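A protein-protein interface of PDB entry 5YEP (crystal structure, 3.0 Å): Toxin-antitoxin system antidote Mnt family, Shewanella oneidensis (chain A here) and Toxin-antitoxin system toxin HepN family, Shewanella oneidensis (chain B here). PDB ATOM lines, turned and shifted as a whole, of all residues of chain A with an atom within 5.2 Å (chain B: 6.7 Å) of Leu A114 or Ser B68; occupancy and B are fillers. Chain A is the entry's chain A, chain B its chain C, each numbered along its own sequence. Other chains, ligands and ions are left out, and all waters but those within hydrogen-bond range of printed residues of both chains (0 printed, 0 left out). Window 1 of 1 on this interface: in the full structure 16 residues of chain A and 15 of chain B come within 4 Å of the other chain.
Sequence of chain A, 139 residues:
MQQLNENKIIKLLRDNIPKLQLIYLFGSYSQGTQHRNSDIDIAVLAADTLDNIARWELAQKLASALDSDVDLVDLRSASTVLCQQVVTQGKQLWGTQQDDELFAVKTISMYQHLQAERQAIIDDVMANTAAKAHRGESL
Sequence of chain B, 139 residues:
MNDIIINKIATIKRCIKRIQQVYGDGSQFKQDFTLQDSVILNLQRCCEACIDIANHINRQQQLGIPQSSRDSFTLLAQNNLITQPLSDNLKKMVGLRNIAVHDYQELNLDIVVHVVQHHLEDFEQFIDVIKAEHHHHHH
The backbone NH of Thr A80 is in hydrogen-bond range of the backbone carbonyl oxygen of Gln B67 (3.0 Å).
The backbone NH (N) of Val A81 is in hydrogen-bond range of the backbone carbonyl oxygen (O) of Gln B67 (3.0 Å).
The side-chain amide nitrogen of Asn B55 is in hydrogen-bond range of the backbone carbonyl oxygen of Glu A117, at 3.4 Å.
The side-chain carboxylate (OE1) of Glu A117 sits at hydrogen-bond distance from the side-chain hydroxyl (OG) of Ser B69 (2.7 Å).
The guanidinium group of Arg A118 lies within hydrogen-bond range of the backbone carbonyl oxygen of Pro B66 (2.9 Å).
The side-chain amide oxygen of Gln A115 lies within hydrogen-bond range of the guanidinium group of Arg A118 (3.0 Å).
OD1 of Asn B55 lies within hydrogen-bond range of OG of Ser B72, 2.5 Å away.
The backbone carbonyl oxygen (O) of Ile B65 is in hydrogen-bond range of the side-chain amide nitrogen (NE2) of Gln B67 (2.8 Å).
N of Gln B67 lies within hydrogen-bond range of OD2 of Asp B71 (3.4 Å).
The side-chain hydroxyl (OG) of Ser B68 lies close to the backbone NH (N) of Arg B70.
The side-chain hydroxyl (OG) of Ser B68 sits at hydrogen-bond distance from the backbone NH (N) of Asp B71 (3.3 Å).
Ser A79 touches Gln B67.
CB of Ser B68 touches OG1 of Thr A80, at 3.2 Å.
His B102 touches Met A110.
His B102 touches His A113 (NE2 to CD2, 3.5 Å).
Gln B67 touches Leu A114 (O to CD2, 3.7 Å).
C of Ser B68 touches CD1 of Leu A114, at 3.7 Å.
Ser B69 touches Leu A114.
Arg A118 touches Ile B65 (NH1 to CG2, 3.8 Å).
Gln B67 touches Arg A118.
Leu A114 touches just these residues of chain B: Gln B67, Ser B68 and Ser B69.
Printed residues of chain A within 4 Å of Ser B68: Thr A80 and Leu A114.
Printed residues of chain B within 4 Å of Glu A117: Asn B55 (3.4 Å) and Ser B69 (2.7 Å).
Of the printed residues of chain A, Ile B65 touches Arg A118 (3.8 Å).
The nearest residue of chain B that does not touch Leu A114 is Pro B66 (4.5 Å).
The nearest residue of chain A that does not touch Ser B68 is Ser A79 (4.4 Å).
The nearest printed residue of chain B that does not touch Arg A118 is Asn B55 (4.8 Å).
Printed residues of chain A that touch a printed residue of chain B: Ser A79, Thr A80, Val A81, Met A110, His A113, Leu A114, Glu A117 and Arg A118.
Hydrophobic or aromatic side chains of chain A within 4 Å of the printed part of chain B: Val A81, Met A110, His A113 and Leu A114.
Of the 12 printed residues of chain B, 7 touch a printed residue of chain A.
Among the printed residues, 14 pairs touch across the chains.
Among the printed residues, no Asp or Glu carboxylate lies within 4 Å of a Lys or Arg side-chain nitrogen of the other chain.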
ATOM      1  N   SER A  79     -10.245  10.493 -20.547  1.00  0.00           N
ATOM      2  CA  SER A  79      -9.666  10.247 -21.858  1.00  0.00           C
ATOM      3  C   SER A  79      -8.279  10.876 -21.960  1.00  0.00           C
ATOM      4  O   SER A  79      -7.922  11.785 -21.207  1.00  0.00           O
ATOM      5  CB  SER A  79     -10.571  10.799 -22.960  1.00  0.00           C
ATOM      6  OG  SER A  79     -10.456  12.207 -23.060  1.00  0.00           O
ATOM      7  N   THR A  80      -7.493  10.377 -22.917  1.00  0.00           N
ATOM      8  CA  THR A  80      -6.126  10.863 -23.076  1.00  0.00           C
ATOM      9  C   THR A  80      -6.105  12.316 -23.532  1.00  0.00           C
ATOM     10  O   THR A  80      -5.233  13.089 -23.118  1.00  0.00           O
ATOM     11  CB  THR A  80      -5.364   9.973 -24.061  1.00  0.00           C
ATOM     12  OG1 THR A  80      -5.531   8.600 -23.692  1.00  0.00           O
ATOM     13  CG2 THR A  80      -3.875  10.315 -24.050  1.00  0.00           C
ATOM     14  N   VAL A  81      -7.056  12.707 -24.383  1.00  0.00           N
ATOM     15  CA  VAL A  81      -7.116  14.088 -24.850  1.00  0.00           C
ATOM     16  C   VAL A  81      -7.478  15.024 -23.704  1.00  0.00           C
ATOM     17  O   VAL A  81      -6.938  16.131 -23.595  1.00  0.00           O
ATOM     18  CB  VAL A  81      -8.108  14.208 -26.019  1.00  0.00           C
ATOM     19  CG1 VAL A  81      -8.199  15.646 -26.491  1.00  0.00           C
ATOM     20  CG2 VAL A  81      -7.688  13.301 -27.159  1.00  0.00           C
ATOM     21  N   MET A 110       1.855   9.268 -23.735  1.00  0.00           N
ATOM     22  CA  MET A 110       0.671   8.570 -24.221  1.00  0.00           C
ATOM     23  C   MET A 110      -0.037   9.387 -25.296  1.00  0.00           C
ATOM     24  O   MET A 110      -0.662   8.833 -26.200  1.00  0.00           O
ATOM     25  CB  MET A 110      -0.296   8.270 -23.073  1.00  0.00           C
ATOM     26  CG  MET A 110       0.101   7.087 -22.207  1.00  0.00           C
ATOM     27  SD  MET A 110      -1.407   6.353 -21.208  1.00  0.00           S
ATOM     28  CE  MET A 110      -2.350   8.019 -20.826  1.00  0.00           C
ATOM     29  N   TYR A 111       0.066  10.714 -25.190  1.00  0.00           N
ATOM     30  CA  TYR A 111      -0.585  11.578 -26.168  1.00  0.00           C
ATOM     31  C   TYR A 111       0.164  11.571 -27.495  1.00  0.00           C
ATOM     32  O   TYR A 111      -0.458  11.529 -28.563  1.00  0.00           O
ATOM     33  CB  TYR A 111      -0.701  13.000 -25.620  1.00  0.00           C
ATOM     34  CG  TYR A 111      -1.471  13.939 -26.518  1.00  0.00           C
ATOM     35  CD1 TYR A 111      -2.860  13.966 -26.503  1.00  0.00           C
ATOM     36  CD2 TYR A 111      -0.808  14.805 -27.378  1.00  0.00           C
ATOM     37  CE1 TYR A 111      -3.566  14.825 -27.323  1.00  0.00           C
ATOM     38  CE2 TYR A 111      -1.505  15.667 -28.199  1.00  0.00           C
ATOM     39  CZ  TYR A 111      -2.882  15.673 -28.169  1.00  0.00           C
ATOM     40  OH  TYR A 111      -3.575  16.534 -28.991  1.00  0.00           O
ATOM     41  N   GLN A 112       1.498  11.609 -27.448  1.00  0.00           N
ATOM     42  CA  GLN A 112       2.281  11.534 -28.678  1.00  0.00           C
ATOM     43  C   GLN A 112       2.031  10.227 -29.417  1.00  0.00           C
ATOM     44  O   GLN A 112       2.127  10.180 -30.648  1.00  0.00           O
ATOM     45  CB  GLN A 112       3.767  11.697 -28.363  1.00  0.00           C
ATOM     46  CG  GLN A 112       4.134  13.069 -27.839  1.00  0.00           C
ATOM     47  CD  GLN A 112       5.446  13.068 -27.087  1.00  0.00           C
ATOM     48  OE1 GLN A 112       5.996  12.010 -26.777  1.00  0.00           O
ATOM     49  NE2 GLN A 112       5.963  14.258 -26.796  1.00  0.00           N
ATOM     50  N   HIS A 113       1.703   9.160 -28.687  1.00  0.00           N
ATOM     51  CA  HIS A 113       1.374   7.892 -29.326  1.00  0.00           C
ATOM     52  C   HIS A 113      -0.045   7.905 -29.877  1.00  0.00           C
ATOM     53  O   HIS A 113      -0.302   7.351 -30.951  1.00  0.00           O
ATOM     54  CB  HIS A 113       1.553   6.742 -28.336  1.00  0.00           C
ATOM     55  CG  HIS A 113       2.966   6.552 -27.879  1.00  0.00           C
ATOM     56  ND1 HIS A 113       3.766   7.597 -27.470  1.00  0.00           N
ATOM     57  CD2 HIS A 113       3.722   5.435 -27.769  1.00  0.00           C
ATOM     58  CE1 HIS A 113       4.953   7.132 -27.129  1.00  0.00           C
ATOM     59  NE2 HIS A 113       4.953   5.823 -27.301  1.00  0.00           N
ATOM     60  N   LEU A 114      -0.973   8.532 -29.151  1.00  0.00           N
ATOM     61  CA  LEU A 114      -2.347   8.642 -29.631  1.00  0.00           C
ATOM     62  C   LEU A 114      -2.421   9.480 -30.900  1.00  0.00           C
ATOM     63  O   LEU A 114      -3.140   9.128 -31.843  1.00  0.00           O
ATOM     64  CB  LEU A 114      -3.230   9.246 -28.543  1.00  0.00           C
ATOM     65  CG  LEU A 114      -4.673   9.559 -28.933  1.00  0.00           C
ATOM     66  CD1 LEU A 114      -5.514   8.288 -29.013  1.00  0.00           C
ATOM     67  CD2 LEU A 114      -5.270  10.560 -27.957  1.00  0.00           C
ATOM     68  N   GLN A 115      -1.689  10.598 -30.939  1.00  0.00           N
ATOM     69  CA  GLN A 115      -1.655  11.422 -32.143  1.00  0.00           C
ATOM     70  C   GLN A 115      -1.180  10.629 -33.350  1.00  0.00           C
ATOM     71  O   GLN A 115      -1.609  10.898 -34.477  1.00  0.00           O
ATOM     72  CB  GLN A 115      -0.753  12.638 -31.927  1.00  0.00           C
ATOM     73  CG  GLN A 115      -1.373  13.748 -31.094  1.00  0.00           C
ATOM     74  CD  GLN A 115      -2.498  14.465 -31.815  1.00  0.00           C
ATOM     75  OE1 GLN A 115      -3.629  13.978 -31.864  1.00  0.00           O
ATOM     76  NE2 GLN A 115      -2.192  15.625 -32.383  1.00  0.00           N
ATOM     77  N   ALA A 116      -0.299   9.649 -33.136  1.00  0.00           N
ATOM     78  CA  ALA A 116       0.150   8.812 -34.241  1.00  0.00           C
ATOM     79  C   ALA A 116      -0.914   7.802 -34.648  1.00  0.00           C
ATOM     80  O   ALA A 116      -0.948   7.374 -35.808  1.00  0.00           O
ATOM     81  CB  ALA A 116       1.448   8.099 -33.863  1.00  0.00           C
ATOM     82  N   GLU A 117      -1.792   7.415 -33.720  1.00  0.00           N
ATOM     83  CA  GLU A 117      -2.809   6.414 -34.022  1.00  0.00           C
ATOM     84  C   GLU A 117      -4.004   7.001 -34.762  1.00  0.00           C
ATOM     85  O   GLU A 117      -4.598   6.319 -35.606  1.00  0.00           O
ATOM     86  CB  GLU A 117      -3.298   5.748 -32.735  1.00  0.00           C
ATOM     87  CG  GLU A 117      -2.252   4.946 -31.985  1.00  0.00           C
ATOM     88  CD  GLU A 117      -2.790   4.397 -30.677  1.00  0.00           C
ATOM     89  OE1 GLU A 117      -3.995   4.586 -30.406  1.00  0.00           O
ATOM     90  OE2 GLU A 117      -2.010   3.781 -29.919  1.00  0.00           O
ATOM     91  N   ARG A 118      -4.372   8.247 -34.466  1.00  0.00           N
ATOM     92  CA  ARG A 118      -5.617   8.828 -34.950  1.00  0.00           C
ATOM     93  C   ARG A 118      -5.408   9.945 -35.965  1.00  0.00           C
ATOM     94  O   ARG A 118      -6.367  10.655 -36.288  1.00  0.00           O
ATOM     95  CB  ARG A 118      -6.442   9.350 -33.772  1.00  0.00           C
ATOM     96  CG  ARG A 118      -5.776  10.492 -33.025  1.00  0.00           C
ATOM     97  CD  ARG A 118      -6.735  11.179 -32.073  1.00  0.00           C
ATOM     98  NE  ARG A 118      -6.194  12.455 -31.615  1.00  0.00           N
ATOM     99  CZ  ARG A 118      -6.851  13.322 -30.851  1.00  0.00           C
ATOM    100  NH1 ARG A 118      -8.089  13.060 -30.456  1.00  0.00           N
ATOM    101  NH2 ARG A 118      -6.269  14.456 -30.490  1.00  0.00           N
ATOM    102  N   GLN A 119      -4.190  10.120 -36.483  1.00  0.00           N
ATOM    103  CA  GLN A 119      -3.952  11.217 -37.418  1.00  0.00           C
ATOM    104  C   GLN A 119      -4.604  10.955 -38.770  1.00  0.00           C
ATOM    105  O   GLN A 119      -4.995  11.903 -39.461  1.00  0.00           O
ATOM    106  CB  GLN A 119      -2.453  11.462 -37.586  1.00  0.00           C
ATOM    107  CG  GLN A 119      -2.115  12.844 -38.138  1.00  0.00           C
ATOM    108  CD  GLN A 119      -2.373  13.966 -37.140  1.00  0.00           C
ATOM    109  OE1 GLN A 119      -2.762  13.726 -35.996  1.00  0.00           O
ATOM    110  NE2 GLN A 119      -2.159  15.203 -37.575  1.00  0.00           N
ATOM    111  N   ASN B  55      -9.565   1.577 -36.093  1.00  0.00           N
ATOM    112  CA  ASN B  55      -9.467   2.947 -36.587  1.00  0.00           C
ATOM    113  C   ASN B  55      -9.733   3.043 -38.085  1.00  0.00           C
ATOM    114  O   ASN B  55     -10.258   4.062 -38.550  1.00  0.00           O
ATOM    115  CB  ASN B  55      -8.091   3.529 -36.261  1.00  0.00           C
ATOM    116  CG  ASN B  55      -7.974   3.982 -34.815  1.00  0.00           C
ATOM    117  OD1 ASN B  55      -8.975   4.250 -34.152  1.00  0.00           O
ATOM    118  ND2 ASN B  55      -6.745   4.074 -34.323  1.00  0.00           N
ATOM    119  N   ILE B  65     -14.187  10.717 -33.351  1.00  0.00           N
ATOM    120  CA  ILE B  65     -12.771  11.021 -33.200  1.00  0.00           C
ATOM    121  C   ILE B  65     -12.300  10.423 -31.879  1.00  0.00           C
ATOM    122  O   ILE B  65     -12.754  10.847 -30.812  1.00  0.00           O
ATOM    123  CB  ILE B  65     -12.495  12.532 -33.238  1.00  0.00           C
ATOM    124  CG1 ILE B  65     -12.787  13.059 -34.643  1.00  0.00           C
ATOM    125  CG2 ILE B  65     -11.063  12.821 -32.805  1.00  0.00           C
ATOM    126  CD1 ILE B  65     -12.106  14.350 -34.965  1.00  0.00           C
ATOM    127  N   PRO B  66     -11.401   9.442 -31.900  1.00  0.00           N
ATOM    128  CA  PRO B  66     -10.990   8.782 -30.653  1.00  0.00           C
ATOM    129  C   PRO B  66     -10.262   9.741 -29.720  1.00  0.00           C
ATOM    130  O   PRO B  66      -9.297  10.403 -30.107  1.00  0.00           O
ATOM    131  CB  PRO B  66     -10.064   7.659 -31.137  1.00  0.00           C
ATOM    132  CG  PRO B  66     -10.434   7.453 -32.578  1.00  0.00           C
ATOM    133  CD  PRO B  66     -10.814   8.805 -33.088  1.00  0.00           C
ATOM    134  N   GLN B  67     -10.746   9.816 -28.483  1.00  0.00           N
ATOM    135  CA  GLN B  67     -10.096  10.597 -27.444  1.00  0.00           C
ATOM    136  C   GLN B  67      -9.062   9.792 -26.669  1.00  0.00           C
ATOM    137  O   GLN B  67      -8.345  10.366 -25.840  1.00  0.00           O
ATOM    138  CB  GLN B  67     -11.147  11.156 -26.480  1.00  0.00           C
ATOM    139  CG  GLN B  67     -12.334  11.800 -27.177  1.00  0.00           C
ATOM    140  CD  GLN B  67     -11.955  13.060 -27.928  1.00  0.00           C
ATOM    141  OE1 GLN B  67     -11.733  14.110 -27.326  1.00  0.00           O
ATOM    142  NE2 GLN B  67     -11.885  12.966 -29.250  1.00  0.00           N
ATOM    143  N   SER B  68      -8.973   8.490 -26.919  1.00  0.00           N
ATOM    144  CA  SER B  68      -7.988   7.612 -26.300  1.00  0.00           C
ATOM    145  C   SER B  68      -7.985   6.312 -27.092  1.00  0.00           C
ATOM    146  O   SER B  68      -8.884   6.055 -27.897  1.00  0.00           O
ATOM    147  CB  SER B  68      -8.297   7.354 -24.822  1.00  0.00           C
ATOM    148  OG  SER B  68      -9.385   6.459 -24.678  1.00  0.00           O
ATOM    149  N   SER B  69      -6.959   5.492 -26.857  1.00  0.00           N
ATOM    150  CA  SER B  69      -6.894   4.201 -27.534  1.00  0.00           C
ATOM    151  C   SER B  69      -8.063   3.308 -27.142  1.00  0.00           C
ATOM    152  O   SER B  69      -8.516   2.487 -27.948  1.00  0.00           O
ATOM    153  CB  SER B  69      -5.566   3.507 -27.231  1.00  0.00           C
ATOM    154  OG  SER B  69      -4.482   4.196 -27.827  1.00  0.00           O
ATOM    155  N   ARG B  70      -8.564   3.452 -25.913  1.00  0.00           N
ATOM    156  CA  ARG B  70      -9.750   2.708 -25.503  1.00  0.00           C
ATOM    157  C   ARG B  70     -10.989   3.173 -26.257  1.00  0.00           C
ATOM    158  O   ARG B  70     -11.908   2.380 -26.487  1.00  0.00           O
ATOM    159  CB  ARG B  70      -9.966   2.859 -23.997  1.00  0.00           C
ATOM    160  CG  ARG B  70      -8.961   2.108 -23.138  1.00  0.00           C
ATOM    161  CD  ARG B  70      -9.061   2.521 -21.673  1.00  0.00           C
ATOM    162  NE  ARG B  70      -8.572   3.879 -21.447  1.00  0.00           N
ATOM    163  CZ  ARG B  70      -9.350   4.954 -21.343  1.00  0.00           C
ATOM    164  NH1 ARG B  70     -10.668   4.838 -21.442  1.00  0.00           N
ATOM    165  NH2 ARG B  70      -8.807   6.146 -21.137  1.00  0.00           N
ATOM    166  N   ASP B  71     -11.025   4.447 -26.653  1.00  0.00           N
ATOM    167  CA  ASP B  71     -12.187   4.991 -27.343  1.00  0.00           C
ATOM    168  C   ASP B  71     -12.381   4.383 -28.727  1.00  0.00           C
ATOM    169  O   ASP B  71     -13.496   4.426 -29.257  1.00  0.00           O
ATOM    170  CB  ASP B  71     -12.055   6.511 -27.453  1.00  0.00           C
ATOM    171  CG  ASP B  71     -13.389   7.223 -27.358  1.00  0.00           C
ATOM    172  OD1 ASP B  71     -14.410   6.636 -27.771  1.00  0.00           O
ATOM    173  OD2 ASP B  71     -13.416   8.373 -26.870  1.00  0.00           O
ATOM    174  N   SER B  72     -11.328   3.812 -29.319  1.00  0.00           N
ATOM    175  CA  SER B  72     -11.442   3.273 -30.671  1.00  0.00           C
ATOM    176  C   SER B  72     -12.339   2.044 -30.722  1.00  0.00           C
ATOM    177  O   SER B  72     -12.920   1.748 -31.772  1.00  0.00           O
ATOM    178  CB  SER B  72     -10.057   2.938 -31.223  1.00  0.00           C
ATOM    179  OG  SER B  72      -9.378   4.108 -31.646  1.00  0.00           O
ATOM    180  N   PHE B  73     -12.462   1.316 -29.613  1.00  0.00           N
ATOM    181  CA  PHE B  73     -13.330   0.148 -29.577  1.00  0.00           C
ATOM    182  C   PHE B  73     -14.734   0.476 -29.093  1.00  0.00           C
ATOM    183  O   PHE B  73     -15.683  -0.234 -29.445  1.00  0.00           O
ATOM    184  CB  PHE B  73     -12.723  -0.941 -28.690  1.00  0.00           C
ATOM    185  CG  PHE B  73     -11.445  -1.509 -29.226  1.00  0.00           C
ATOM    186  CD1 PHE B  73     -11.459  -2.368 -30.312  1.00  0.00           C
ATOM    187  CD2 PHE B  73     -10.230  -1.190 -28.646  1.00  0.00           C
ATOM    188  CE1 PHE B  73     -10.285  -2.893 -30.812  1.00  0.00           C
ATOM    189  CE2 PHE B  73      -9.051  -1.713 -29.139  1.00  0.00           C
ATOM    190  CZ  PHE B  73      -9.078  -2.566 -30.224  1.00  0.00           C
ATOM    191  N   VAL B  94      -6.110  -2.881 -23.943  1.00  0.00           N
ATOM    192  CA  VAL B  94      -5.437  -1.597 -24.115  1.00  0.00           C
ATOM    193  C   VAL B  94      -4.847  -1.131 -22.790  1.00  0.00           C
ATOM    194  O   VAL B  94      -3.766  -0.532 -22.752  1.00  0.00           O
ATOM    195  CB  VAL B  94      -6.411  -0.563 -24.708  1.00  0.00           C
ATOM    196  CG1 VAL B  94      -5.728   0.786 -24.875  1.00  0.00           C
ATOM    197  CG2 VAL B  94      -6.950  -1.054 -26.042  1.00  0.00           C
ATOM    198  N   HIS B 102       3.973   2.340 -21.806  1.00  0.00           N
ATOM    199  CA  HIS B 102       4.265   3.476 -20.923  1.00  0.00           C
ATOM    200  C   HIS B 102       4.339   2.915 -19.515  1.00  0.00           C
ATOM    201  O   HIS B 102       3.508   2.101 -19.102  1.00  0.00           O
ATOM    202  CB  HIS B 102       3.201   4.556 -21.026  1.00  0.00           C
ATOM    203  CG  HIS B 102       2.851   4.936 -22.432  1.00  0.00           C
ATOM    204  ND1 HIS B 102       1.804   4.360 -23.119  1.00  0.00           N
ATOM    205  CD2 HIS B 102       3.419   5.822 -23.283  1.00  0.00           C
ATOM    206  CE1 HIS B 102       1.734   4.886 -24.330  1.00  0.00           C
ATOM    207  NE2 HIS B 102       2.703   5.774 -24.455  1.00  0.00           N
